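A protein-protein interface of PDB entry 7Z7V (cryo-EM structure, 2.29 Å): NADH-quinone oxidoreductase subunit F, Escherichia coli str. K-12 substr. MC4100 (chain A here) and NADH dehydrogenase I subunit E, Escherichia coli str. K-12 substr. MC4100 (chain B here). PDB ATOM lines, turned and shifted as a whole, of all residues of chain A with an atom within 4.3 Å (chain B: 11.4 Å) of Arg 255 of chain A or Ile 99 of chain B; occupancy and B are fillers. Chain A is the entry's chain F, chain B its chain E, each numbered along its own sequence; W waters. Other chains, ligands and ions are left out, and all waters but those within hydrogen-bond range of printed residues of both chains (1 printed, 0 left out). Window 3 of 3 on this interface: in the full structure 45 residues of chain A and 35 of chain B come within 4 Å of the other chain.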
ATOM      1  N   GLY A 254       1.151  17.174  19.141  1.00  0.00           N
ATOM      2  CA  GLY A 254       1.253  18.616  19.224  1.00  0.00           C
ATOM      3  C   GLY A 254       1.886  19.125  20.499  1.00  0.00           C
ATOM      4  O   GLY A 254       1.203  19.302  21.511  1.00  0.00           O
ATOM      5  N   ARG A 255       3.191  19.397  20.428  1.00  0.00           N
ATOM      6  CA  ARG A 255       3.975  20.013  21.505  1.00  0.00           C
ATOM      7  C   ARG A 255       3.855  19.252  22.823  1.00  0.00           C
ATOM      8  O   ARG A 255       3.808  19.840  23.904  1.00  0.00           O
ATOM      9  CB  ARG A 255       3.602  21.483  21.676  1.00  0.00           C
ATOM     10  CG  ARG A 255       3.857  22.291  20.422  1.00  0.00           C
ATOM     11  CD  ARG A 255       4.676  23.522  20.704  1.00  0.00           C
ATOM     12  NE  ARG A 255       3.840  24.643  21.110  1.00  0.00           N
ATOM     13  CZ  ARG A 255       4.187  25.914  20.981  1.00  0.00           C
ATOM     14  NH1 ARG A 255       5.349  26.262  20.455  1.00  0.00           N
ATOM     15  NH2 ARG A 255       3.347  26.860  21.388  1.00  0.00           N
ATOM     16  N   VAL A 256       3.808  17.932  22.728  1.00  0.00           N
ATOM     17  CA  VAL A 256       3.933  17.072  23.879  1.00  0.00           C
ATOM     18  C   VAL A 256       5.339  16.489  23.875  1.00  0.00           C
ATOM     19  O   VAL A 256       6.084  16.618  22.907  1.00  0.00           O
ATOM     20  CB  VAL A 256       2.853  15.963  23.897  1.00  0.00           C
ATOM     21  CG1 VAL A 256       1.536  16.521  24.387  1.00  0.00           C
ATOM     22  CG2 VAL A 256       2.694  15.355  22.524  1.00  0.00           C
ATOM     23  N   MET A 281       2.922  17.677  28.459  1.00  0.00           N
ATOM     24  CA  MET A 281       3.365  18.777  27.623  1.00  0.00           C
ATOM     25  C   MET A 281       4.867  18.991  27.774  1.00  0.00           C
ATOM     26  O   MET A 281       5.493  18.538  28.735  1.00  0.00           O
ATOM     27  CB  MET A 281       2.611  20.059  27.973  1.00  0.00           C
ATOM     28  CG  MET A 281       1.116  19.863  28.122  1.00  0.00           C
ATOM     29  SD  MET A 281       0.213  19.911  26.561  1.00  0.00           S
ATOM     30  CE  MET A 281       1.209  21.028  25.582  1.00  0.00           C
ATOM     31  N   ARG A 282       5.444  19.683  26.798  1.00  0.00           N
ATOM     32  CA  ARG A 282       6.857  20.011  26.846  1.00  0.00           C
ATOM     33  C   ARG A 282       7.130  21.021  27.956  1.00  0.00           C
ATOM     34  O   ARG A 282       6.221  21.682  28.468  1.00  0.00           O
ATOM     35  CB  ARG A 282       7.325  20.564  25.502  1.00  0.00           C
ATOM     36  CG  ARG A 282       7.171  19.589  24.353  1.00  0.00           C
ATOM     37  CD  ARG A 282       8.308  19.723  23.360  1.00  0.00           C
ATOM     38  NE  ARG A 282       8.313  21.028  22.713  1.00  0.00           N
ATOM     39  CZ  ARG A 282       7.882  21.253  21.480  1.00  0.00           C
ATOM     40  NH1 ARG A 282       7.396  20.280  20.728  1.00  0.00           N
ATOM     41  NH2 ARG A 282       7.942  22.487  20.988  1.00  0.00           N
ATOM     42  N   LEU A 285       5.543  24.767  28.701  1.00  0.00           N
ATOM     43  CA  LEU A 285       4.229  24.867  28.086  1.00  0.00           C
ATOM     44  C   LEU A 285       3.169  24.337  29.039  1.00  0.00           C
ATOM     45  O   LEU A 285       3.374  23.322  29.710  1.00  0.00           O
ATOM     46  CB  LEU A 285       4.178  24.092  26.768  1.00  0.00           C
ATOM     47  CG  LEU A 285       5.145  24.561  25.681  1.00  0.00           C
ATOM     48  CD1 LEU A 285       5.191  23.561  24.543  1.00  0.00           C
ATOM     49  CD2 LEU A 285       4.745  25.933  25.172  1.00  0.00           C
ATOM     50  N   MET A 327      -5.247  15.886  19.844  1.00  0.00           N
ATOM     51  CA  MET A 327      -4.280  16.949  19.635  1.00  0.00           C
ATOM     52  C   MET A 327      -4.321  17.879  20.837  1.00  0.00           C
ATOM     53  O   MET A 327      -5.398  18.330  21.236  1.00  0.00           O
ATOM     54  CB  MET A 327      -4.578  17.720  18.348  1.00  0.00           C
ATOM     55  CG  MET A 327      -3.714  18.941  18.137  1.00  0.00           C
ATOM     56  SD  MET A 327      -4.294  19.943  16.761  1.00  0.00           S
ATOM     57  CE  MET A 327      -5.622  20.839  17.558  1.00  0.00           C
ATOM     58  N   ALA A 328      -3.154  18.152  21.408  1.00  0.00           N
ATOM     59  CA  ALA A 328      -3.039  19.045  22.549  1.00  0.00           C
ATOM     60  C   ALA A 328      -2.720  20.458  22.082  1.00  0.00           C
ATOM     61  O   ALA A 328      -1.900  20.660  21.186  1.00  0.00           O
ATOM     62  CB  ALA A 328      -1.958  18.559  23.512  1.00  0.00           C
ATOM     63  N   VAL A 329      -3.379  21.431  22.700  1.00  0.00           N
ATOM     64  CA  VAL A 329      -3.188  22.845  22.422  1.00  0.00           C
ATOM     65  C   VAL A 329      -2.646  23.477  23.692  1.00  0.00           C
ATOM     66  O   VAL A 329      -3.299  23.419  24.743  1.00  0.00           O
ATOM     67  CB  VAL A 329      -4.500  23.520  21.996  1.00  0.00           C
ATOM     68  CG1 VAL A 329      -4.263  24.967  21.636  1.00  0.00           C
ATOM     69  CG2 VAL A 329      -5.133  22.768  20.841  1.00  0.00           C
ATOM     70  N   ASP A 330      -1.463  24.080  23.596  1.00  0.00           N
ATOM     71  CA  ASP A 330      -0.812  24.698  24.736  1.00  0.00           C
ATOM     72  C   ASP A 330      -1.266  26.148  24.886  1.00  0.00           C
ATOM     73  O   ASP A 330      -2.028  26.678  24.076  1.00  0.00           O
ATOM     74  CB  ASP A 330       0.707  24.609  24.601  1.00  0.00           C
ATOM     75  CG  ASP A 330       1.197  25.010  23.229  1.00  0.00           C
ATOM     76  OD1 ASP A 330       1.108  24.184  22.300  1.00  0.00           O
ATOM     77  OD2 ASP A 330       1.680  26.150  23.077  1.00  0.00           O
ATOM     78  N   GLU A 332       0.391  28.888  24.583  1.00  0.00           N
ATOM     79  CA  GLU A 332       0.984  29.835  23.650  1.00  0.00           C
ATOM     80  C   GLU A 332       0.250  29.897  22.320  1.00  0.00           C
ATOM     81  O   GLU A 332       0.607  30.721  21.472  1.00  0.00           O
ATOM     82  CB  GLU A 332       2.452  29.482  23.408  1.00  0.00           C
ATOM     83  CG  GLU A 332       3.278  29.390  24.673  1.00  0.00           C
ATOM     84  CD  GLU A 332       4.761  29.518  24.407  1.00  0.00           C
ATOM     85  OE1 GLU A 332       5.218  29.055  23.342  1.00  0.00           O
ATOM     86  OE2 GLU A 332       5.474  30.078  25.266  1.00  0.00           O
ATOM     87  N   ILE A 333      -0.754  29.056  22.115  1.00  0.00           N
ATOM     88  CA  ILE A 333      -1.497  29.016  20.863  1.00  0.00           C
ATOM     89  C   ILE A 333      -2.732  29.893  21.005  1.00  0.00           C
ATOM     90  O   ILE A 333      -3.565  29.668  21.888  1.00  0.00           O
ATOM     91  CB  ILE A 333      -1.884  27.578  20.494  1.00  0.00           C
ATOM     92  CG1 ILE A 333      -0.636  26.705  20.354  1.00  0.00           C
ATOM     93  CG2 ILE A 333      -2.713  27.564  19.223  1.00  0.00           C
ATOM     94  CD1 ILE A 333       0.256  27.100  19.207  1.00  0.00           C
ATOM     95  N   LEU A 338      -5.875  29.377  15.572  1.00  0.00           N
ATOM     96  CA  LEU A 338      -6.037  27.937  15.397  1.00  0.00           C
ATOM     97  C   LEU A 338      -7.327  27.606  14.658  1.00  0.00           C
ATOM     98  O   LEU A 338      -7.330  26.812  13.707  1.00  0.00           O
ATOM     99  CB  LEU A 338      -6.014  27.250  16.759  1.00  0.00           C
ATOM    100  CG  LEU A 338      -5.687  25.765  16.747  1.00  0.00           C
ATOM    101  CD1 LEU A 338      -4.233  25.584  16.417  1.00  0.00           C
ATOM    102  CD2 LEU A 338      -6.014  25.154  18.087  1.00  0.00           C
ATOM    103  N   CYS B  92       2.938  21.255   4.658  1.00  0.00           N
ATOM    104  CA  CYS B  92       1.674  21.100   5.360  1.00  0.00           C
ATOM    105  C   CYS B  92       1.320  22.382   6.100  1.00  0.00           C
ATOM    106  O   CYS B  92       2.138  22.930   6.842  1.00  0.00           O
ATOM    107  CB  CYS B  92       1.750  19.932   6.336  1.00  0.00           C
ATOM    108  SG  CYS B  92       0.255  19.706   7.293  1.00  0.00           S
ATOM    109  N   ASP B  93       0.095  22.866   5.894  1.00  0.00           N
ATOM    110  CA  ASP B  93      -0.390  24.051   6.588  1.00  0.00           C
ATOM    111  C   ASP B  93      -1.593  23.739   7.472  1.00  0.00           C
ATOM    112  O   ASP B  93      -2.377  24.637   7.787  1.00  0.00           O
ATOM    113  CB  ASP B  93      -0.704  25.173   5.589  1.00  0.00           C
ATOM    114  CG  ASP B  93      -1.925  24.900   4.727  1.00  0.00           C
ATOM    115  OD1 ASP B  93      -2.277  23.730   4.499  1.00  0.00           O
ATOM    116  OD2 ASP B  93      -2.535  25.880   4.260  1.00  0.00           O
ATOM    117  N   SER B  94      -1.743  22.486   7.892  1.00  0.00           N
ATOM    118  CA  SER B  94      -2.876  22.066   8.698  1.00  0.00           C
ATOM    119  C   SER B  94      -2.598  22.332  10.178  1.00  0.00           C
ATOM    120  O   SER B  94      -1.590  22.941  10.542  1.00  0.00           O
ATOM    121  CB  SER B  94      -3.203  20.604   8.421  1.00  0.00           C
ATOM    122  OG  SER B  94      -4.040  20.489   7.287  1.00  0.00           O
ATOM    123  N   VAL B  95      -3.491  21.853  11.047  1.00  0.00           N
ATOM    124  CA  VAL B  95      -3.601  22.402  12.397  1.00  0.00           C
ATOM    125  C   VAL B  95      -2.443  21.954  13.290  1.00  0.00           C
ATOM    126  O   VAL B  95      -1.906  22.752  14.068  1.00  0.00           O
ATOM    127  CB  VAL B  95      -4.984  22.061  12.996  1.00  0.00           C
ATOM    128  CG1 VAL B  95      -5.258  20.560  13.010  1.00  0.00           C
ATOM    129  CG2 VAL B  95      -5.148  22.660  14.369  1.00  0.00           C
ATOM    130  N   VAL B  96      -2.028  20.688  13.194  1.00  0.00           N
ATOM    131  CA  VAL B  96      -0.960  20.202  14.063  1.00  0.00           C
ATOM    132  C   VAL B  96       0.377  20.806  13.658  1.00  0.00           C
ATOM    133  O   VAL B  96       1.183  21.187  14.513  1.00  0.00           O
ATOM    134  CB  VAL B  96      -0.911  18.666  14.065  1.00  0.00           C
ATOM    135  CG1 VAL B  96      -0.048  18.172  15.208  1.00  0.00           C
ATOM    136  CG2 VAL B  96      -2.308  18.095  14.165  1.00  0.00           C
ATOM    137  N   CYS B  97       0.630  20.912  12.355  1.00  0.00           N
ATOM    138  CA  CYS B  97       1.830  21.594  11.894  1.00  0.00           C
ATOM    139  C   CYS B  97       1.766  23.094  12.146  1.00  0.00           C
ATOM    140  O   CYS B  97       2.815  23.735  12.249  1.00  0.00           O
ATOM    141  CB  CYS B  97       2.060  21.305  10.412  1.00  0.00           C
ATOM    142  SG  CYS B  97       2.459  19.579  10.074  1.00  0.00           S
ATOM    143  N   HIS B  98       0.563  23.665  12.240  1.00  0.00           N
ATOM    144  CA  HIS B  98       0.428  25.042  12.704  1.00  0.00           C
ATOM    145  C   HIS B  98       0.847  25.173  14.160  1.00  0.00           C
ATOM    146  O   HIS B  98       1.519  26.140  14.533  1.00  0.00           O
ATOM    147  CB  HIS B  98      -1.009  25.522  12.507  1.00  0.00           C
ATOM    148  CG  HIS B  98      -1.284  26.865  13.107  1.00  0.00           C
ATOM    149  ND1 HIS B  98      -1.752  27.025  14.392  1.00  0.00           N
ATOM    150  CD2 HIS B  98      -1.162  28.111  12.595  1.00  0.00           C
ATOM    151  CE1 HIS B  98      -1.903  28.311  14.647  1.00  0.00           C
ATOM    152  NE2 HIS B  98      -1.554  28.992  13.572  1.00  0.00           N
ATOM    153  N   ILE B  99       0.449  24.212  14.994  1.00  0.00           N
ATOM    154  CA  ILE B  99       0.888  24.194  16.386  1.00  0.00           C
ATOM    155  C   ILE B  99       2.392  23.969  16.468  1.00  0.00           C
ATOM    156  O   ILE B  99       3.095  24.639  17.233  1.00  0.00           O
ATOM    157  CB  ILE B  99       0.094  23.132  17.168  1.00  0.00           C
ATOM    158  CG1 ILE B  99      -1.331  23.621  17.407  1.00  0.00           C
ATOM    159  CG2 ILE B  99       0.759  22.803  18.485  1.00  0.00           C
ATOM    160  CD1 ILE B  99      -2.205  22.646  18.141  1.00  0.00           C
ATOM    161  N   ASN B 100       2.916  23.058  15.653  1.00  0.00           N
ATOM    162  CA  ASN B 100       4.342  22.761  15.633  1.00  0.00           C
ATOM    163  C   ASN B 100       5.161  23.803  14.884  1.00  0.00           C
ATOM    164  O   ASN B 100       6.387  23.677  14.828  1.00  0.00           O
ATOM    165  CB  ASN B 100       4.578  21.380  15.022  1.00  0.00           C
ATOM    166  CG  ASN B 100       4.181  20.262  15.955  1.00  0.00           C
ATOM    167  OD1 ASN B 100       3.525  19.306  15.554  1.00  0.00           O
ATOM    168  ND2 ASN B 100       4.572  20.381  17.214  1.00  0.00           N
ATOM    169  N   GLY B 101       4.526  24.815  14.303  1.00  0.00           N
ATOM    170  CA  GLY B 101       5.250  25.923  13.717  1.00  0.00           C
ATOM    171  C   GLY B 101       5.615  25.759  12.259  1.00  0.00           C
ATOM    172  O   GLY B 101       6.788  25.882  11.897  1.00  0.00           O
ATOM    173  N   TYR B 102       4.626  25.489  11.405  1.00  0.00           N
ATOM    174  CA  TYR B 102       4.888  25.472   9.972  1.00  0.00           C
ATOM    175  C   TYR B 102       5.155  26.862   9.418  1.00  0.00           C
ATOM    176  O   TYR B 102       5.672  26.968   8.306  1.00  0.00           O
ATOM    177  CB  TYR B 102       3.727  24.821   9.202  1.00  0.00           C
ATOM    178  CG  TYR B 102       2.638  25.776   8.736  1.00  0.00           C
ATOM    179  CD1 TYR B 102       1.583  26.096   9.569  1.00  0.00           C
ATOM    180  CD2 TYR B 102       2.662  26.351   7.466  1.00  0.00           C
ATOM    181  CE1 TYR B 102       0.590  26.956   9.170  1.00  0.00           C
ATOM    182  CE2 TYR B 102       1.686  27.230   7.069  1.00  0.00           C
ATOM    183  CZ  TYR B 102       0.643  27.519   7.920  1.00  0.00           C
ATOM    184  OH  TYR B 102      -0.350  28.381   7.527  1.00  0.00           O
ATOM    185  N   GLN B 103       4.768  27.921  10.136  1.00  0.00           N
ATOM    186  CA  GLN B 103       4.913  29.271   9.600  1.00  0.00           C
ATOM    187  C   GLN B 103       6.377  29.656   9.442  1.00  0.00           C
ATOM    188  O   GLN B 103       6.741  30.331   8.474  1.00  0.00           O
ATOM    189  CB  GLN B 103       4.188  30.274  10.492  1.00  0.00           C
ATOM    190  CG  GLN B 103       2.746  30.504  10.102  1.00  0.00           C
ATOM    191  CD  GLN B 103       1.779  30.013  11.151  1.00  0.00           C
ATOM    192  OE1 GLN B 103       2.038  29.025  11.837  1.00  0.00           O
ATOM    193  NE2 GLN B 103       0.657  30.707  11.289  1.00  0.00           N
ATOM    194  N   GLY B 104       7.230  29.228  10.373  1.00  0.00           N
ATOM    195  CA  GLY B 104       8.659  29.442  10.207  1.00  0.00           C
ATOM    196  C   GLY B 104       9.225  28.695   9.015  1.00  0.00           C
ATOM    197  O   GLY B 104      10.080  29.214   8.297  1.00  0.00           O
ATOM    198  N   ILE B 105       8.741  27.472   8.782  1.00  0.00           N
ATOM    199  CA  ILE B 105       9.164  26.693   7.622  1.00  0.00           C
ATOM    200  C   ILE B 105       8.727  27.371   6.332  1.00  0.00           C
ATOM    201  O   ILE B 105       9.495  27.459   5.365  1.00  0.00           O
ATOM    202  CB  ILE B 105       8.602  25.263   7.715  1.00  0.00           C
ATOM    203  CG1 ILE B 105       8.879  24.666   9.095  1.00  0.00           C
ATOM    204  CG2 ILE B 105       9.160  24.398   6.603  1.00  0.00           C
ATOM    205  CD1 ILE B 105      10.331  24.614   9.452  1.00  0.00           C
ATOM    206  N   CYS B 133      -3.116  18.178   5.529  1.00  0.00           N
ATOM    207  CA  CYS B 133      -2.346  17.346   6.445  1.00  0.00           C
ATOM    208  C   CYS B 133      -1.819  16.097   5.756  1.00  0.00           C
ATOM    209  O   CYS B 133      -2.558  15.390   5.066  1.00  0.00           O
ATOM    210  CB  CYS B 133      -3.210  16.961   7.637  1.00  0.00           C
ATOM    211  SG  CYS B 133      -2.668  15.503   8.526  1.00  0.00           S
ATOM    212  N   ASN B 136       1.229  12.860   9.050  1.00  0.00           N
ATOM    213  CA  ASN B 136       2.496  12.700   9.748  1.00  0.00           C
ATOM    214  C   ASN B 136       2.575  13.690  10.894  1.00  0.00           C
ATOM    215  O   ASN B 136       3.626  14.283  11.155  1.00  0.00           O
ATOM    216  CB  ASN B 136       3.670  12.885   8.791  1.00  0.00           C
ATOM    217  CG  ASN B 136       4.800  11.929   9.066  1.00  0.00           C
ATOM    218  OD1 ASN B 136       4.583  10.810   9.524  1.00  0.00           O
ATOM    219  ND2 ASN B 136       6.018  12.364   8.793  1.00  0.00           N
ATOM    220  N   CYS B 137       1.456  13.878  11.593  1.00  0.00           N
ATOM    221  CA  CYS B 137       1.309  15.023  12.486  1.00  0.00           C
ATOM    222  C   CYS B 137       2.144  14.888  13.750  1.00  0.00           C
ATOM    223  O   CYS B 137       2.515  15.902  14.350  1.00  0.00           O
ATOM    224  CB  CYS B 137      -0.162  15.214  12.837  1.00  0.00           C
ATOM    225  SG  CYS B 137      -1.265  14.757  11.504  1.00  0.00           S
ATOM    226  N   ASP B 138       2.451  13.662  14.172  1.00  0.00           N
ATOM    227  CA  ASP B 138       3.280  13.478  15.355  1.00  0.00           C
ATOM    228  C   ASP B 138       4.734  13.853  15.108  1.00  0.00           C
ATOM    229  O   ASP B 138       5.471  14.086  16.069  1.00  0.00           O
ATOM    230  CB  ASP B 138       3.191  12.032  15.845  1.00  0.00           C
ATOM    231  CG  ASP B 138       3.415  11.028  14.738  1.00  0.00           C
ATOM    232  OD1 ASP B 138       3.124  11.349  13.571  1.00  0.00           O
ATOM    233  OD2 ASP B 138       3.883   9.914  15.034  1.00  0.00           O
ATOM    234  N   LYS B 139       5.162  13.915  13.849  1.00  0.00           N
ATOM    235  CA  LYS B 139       6.526  14.275  13.491  1.00  0.00           C
ATOM    236  C   LYS B 139       6.589  15.619  12.771  1.00  0.00           C
ATOM    237  O   LYS B 139       7.514  15.874  12.001  1.00  0.00           O
ATOM    238  CB  LYS B 139       7.155  13.183  12.632  1.00  0.00           C
ATOM    239  CG  LYS B 139       6.817  11.773  13.075  1.00  0.00           C
ATOM    240  CD  LYS B 139       7.110  10.774  11.976  1.00  0.00           C
ATOM    241  CE  LYS B 139       7.300   9.378  12.533  1.00  0.00           C
ATOM    242  NZ  LYS B 139       6.141   8.951  13.353  1.00  0.00           N
ATOM    243  N   GLY B 140       5.614  16.486  13.021  1.00  0.00           N
ATOM    244  CA  GLY B 140       5.523  17.751  12.337  1.00  0.00           C
ATOM    245  C   GLY B 140       6.563  18.757  12.786  1.00  0.00           C
ATOM    246  O   GLY B 140       7.209  18.587  13.822  1.00  0.00           O
ATOM    247  N   PRO B 141       6.747  19.840  12.011  1.00  0.00           N
ATOM    248  CA  PRO B 141       6.078  20.145  10.740  1.00  0.00           C
ATOM    249  C   PRO B 141       6.627  19.336   9.565  1.00  0.00           C
ATOM    250  O   PRO B 141       7.774  18.908   9.597  1.00  0.00           O
ATOM    251  CB  PRO B 141       6.351  21.637  10.555  1.00  0.00           C
ATOM    252  CG  PRO B 141       7.613  21.872  11.272  1.00  0.00           C
ATOM    253  CD  PRO B 141       7.624  20.939  12.444  1.00  0.00           C
ATOM    254  N   ASN B 142       5.799  19.126   8.550  1.00  0.00           N
ATOM    255  CA  ASN B 142       6.100  18.201   7.471  1.00  0.00           C
ATOM    256  C   ASN B 142       6.070  18.913   6.129  1.00  0.00           C
ATOM    257  O   ASN B 142       5.331  19.881   5.935  1.00  0.00           O
ATOM    258  CB  ASN B 142       5.103  17.039   7.440  1.00  0.00           C
ATOM    259  CG  ASN B 142       5.160  16.192   8.682  1.00  0.00           C
ATOM    260  OD1 ASN B 142       6.079  15.404   8.860  1.00  0.00           O
ATOM    261  ND2 ASN B 142       4.169  16.339   9.547  1.00  0.00           N
ATOM    262  N   HIS B 152      10.030  16.690  10.975  1.00  0.00           N
ATOM    263  CA  HIS B 152      10.807  17.376  12.013  1.00  0.00           C
ATOM    264  C   HIS B 152      11.534  18.594  11.455  1.00  0.00           C
ATOM    265  O   HIS B 152      12.714  18.822  11.730  1.00  0.00           O
ATOM    266  CB  HIS B 152      11.789  16.421  12.693  1.00  0.00           C
ATOM    267  CG  HIS B 152      11.145  15.192  13.252  1.00  0.00           C
ATOM    268  ND1 HIS B 152      10.394  15.206  14.406  1.00  0.00           N
ATOM    269  CD2 HIS B 152      11.140  13.911  12.814  1.00  0.00           C
ATOM    270  CE1 HIS B 152       9.955  13.987  14.656  1.00  0.00           C
ATOM    271  NE2 HIS B 152      10.393  13.183  13.706  1.00  0.00           N
ATOM    272  N   LEU B 153      10.822  19.379  10.654  1.00  0.00           N
ATOM    273  CA  LEU B 153      11.448  20.472   9.928  1.00  0.00           C
ATOM    274  C   LEU B 153      11.815  21.619  10.858  1.00  0.00           C
ATOM    275  O   LEU B 153      11.092  21.934  11.806  1.00  0.00           O
ATOM    276  CB  LEU B 153      10.521  20.981   8.831  1.00  0.00           C
ATOM    277  CG  LEU B 153      10.211  20.025   7.688  1.00  0.00           C
ATOM    278  CD1 LEU B 153       9.209  20.669   6.768  1.00  0.00           C
ATOM    279  CD2 LEU B 153      11.470  19.659   6.946  1.00  0.00           C
HETATM  280  O   HOH W   1       2.843  16.679  17.036  1.00  0.00           O
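Gly 254 of chain A touches none of the printed residues of chain B.
Of chain B, only Ile 99 and Asn 100 come within 4 Å of Arg 255 of chain A.
No residue of chain B comes within 4 Å of Val 256 of chain A.
No residue of chain B comes within 4 Å of Leu 285 of chain A.
Of the printed residues of chain B, Met 327 of chain A touches Val 95 (3.7 Å), Val 96 (3.8 Å) and Ile 99 (3.7 Å).
Asp 330 of chain A touches none of the printed residues of chain B.
Of the printed residues of chain B, Leu 338 of chain A touches Val 95, His 98 and Ile 99.
Of the printed residues of chain A, Val 96 of chain B touches Met 327.
Printed residues of chain A within 4 Å of His 98 of chain B: Leu 338 (3.5 Å).
Of the printed residues of chain A, Ile 99 of chain B touches Arg 255, Met 327, Ala 328, Val 329 and Leu 338.
Printed residues of chain A within 4 Å of Asn 100 of chain B: Arg 255 (3.6 Å).
Ile 105 of chain B touches none of the printed residues of chain A.
The nearest printed residue of chain A that does not touch Ile 99 of chain B is Asp 330 of chain A (4.1 Å).
Water W1 lies within hydrogen-bond range of N of Gly 254 of chain A (2.7 Å), O of Cys 137 of chain B (2.8 Å) and OD1 of Asn 100 of chain B (3.1 Å).
Among the printed residues, pairs that only touch across the chains: Leu 338 of chain A with His 98 of chain B (3.5 Å), Arg 255 of chain A with Asn 100 of chain B (3.6 Å), Leu 338 of chain A with Ile 99 of chain B (3.6 Å), Ala 328 of chain A with Ile 99 of chain B (3.6 Å), Met 327 of chain A with Ile 99 of chain B (3.7 Å), Leu 338 of chain A with Val 95 of chain B (3.7 Å), Arg 255 of chain A with Ile 99 of chain B (3.7 Å), Met 327 of chain A with Val 95 of chain B (3.7 Å), Met 327 of chain A with Val 96 of chain B (3.8 Å) and Val 329 of chain A with Ile 99 of chain B (3.98 Å).
The backbone carbonyl oxygen of Arg 255 of chain A sits at hydrogen-bond distance from the backbone NH of Arg 282 of chain A (3.3 Å).
OD2 of Asp 330 of chain A is in salt-bridge range of NH2 of Arg 255 of chain A (2.5 Å).
OE1 of Glu 332 of chain A is in salt-bridge range of NH2 of Arg 255 of chain A (3.5 Å).
O of Val 96 of chain B sits close to OD1 of Asn 100 of chain B (3.2 Å).
Printed residues of chain B that touch a printed residue of chain A: Val 95, Val 96, His 98, Ile 99 and Asn 100.
Along chain B the printed residues that touch a printed residue of chain A span positions 95 to 100.
Among the printed residues, 10 pairs touch across the chains.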
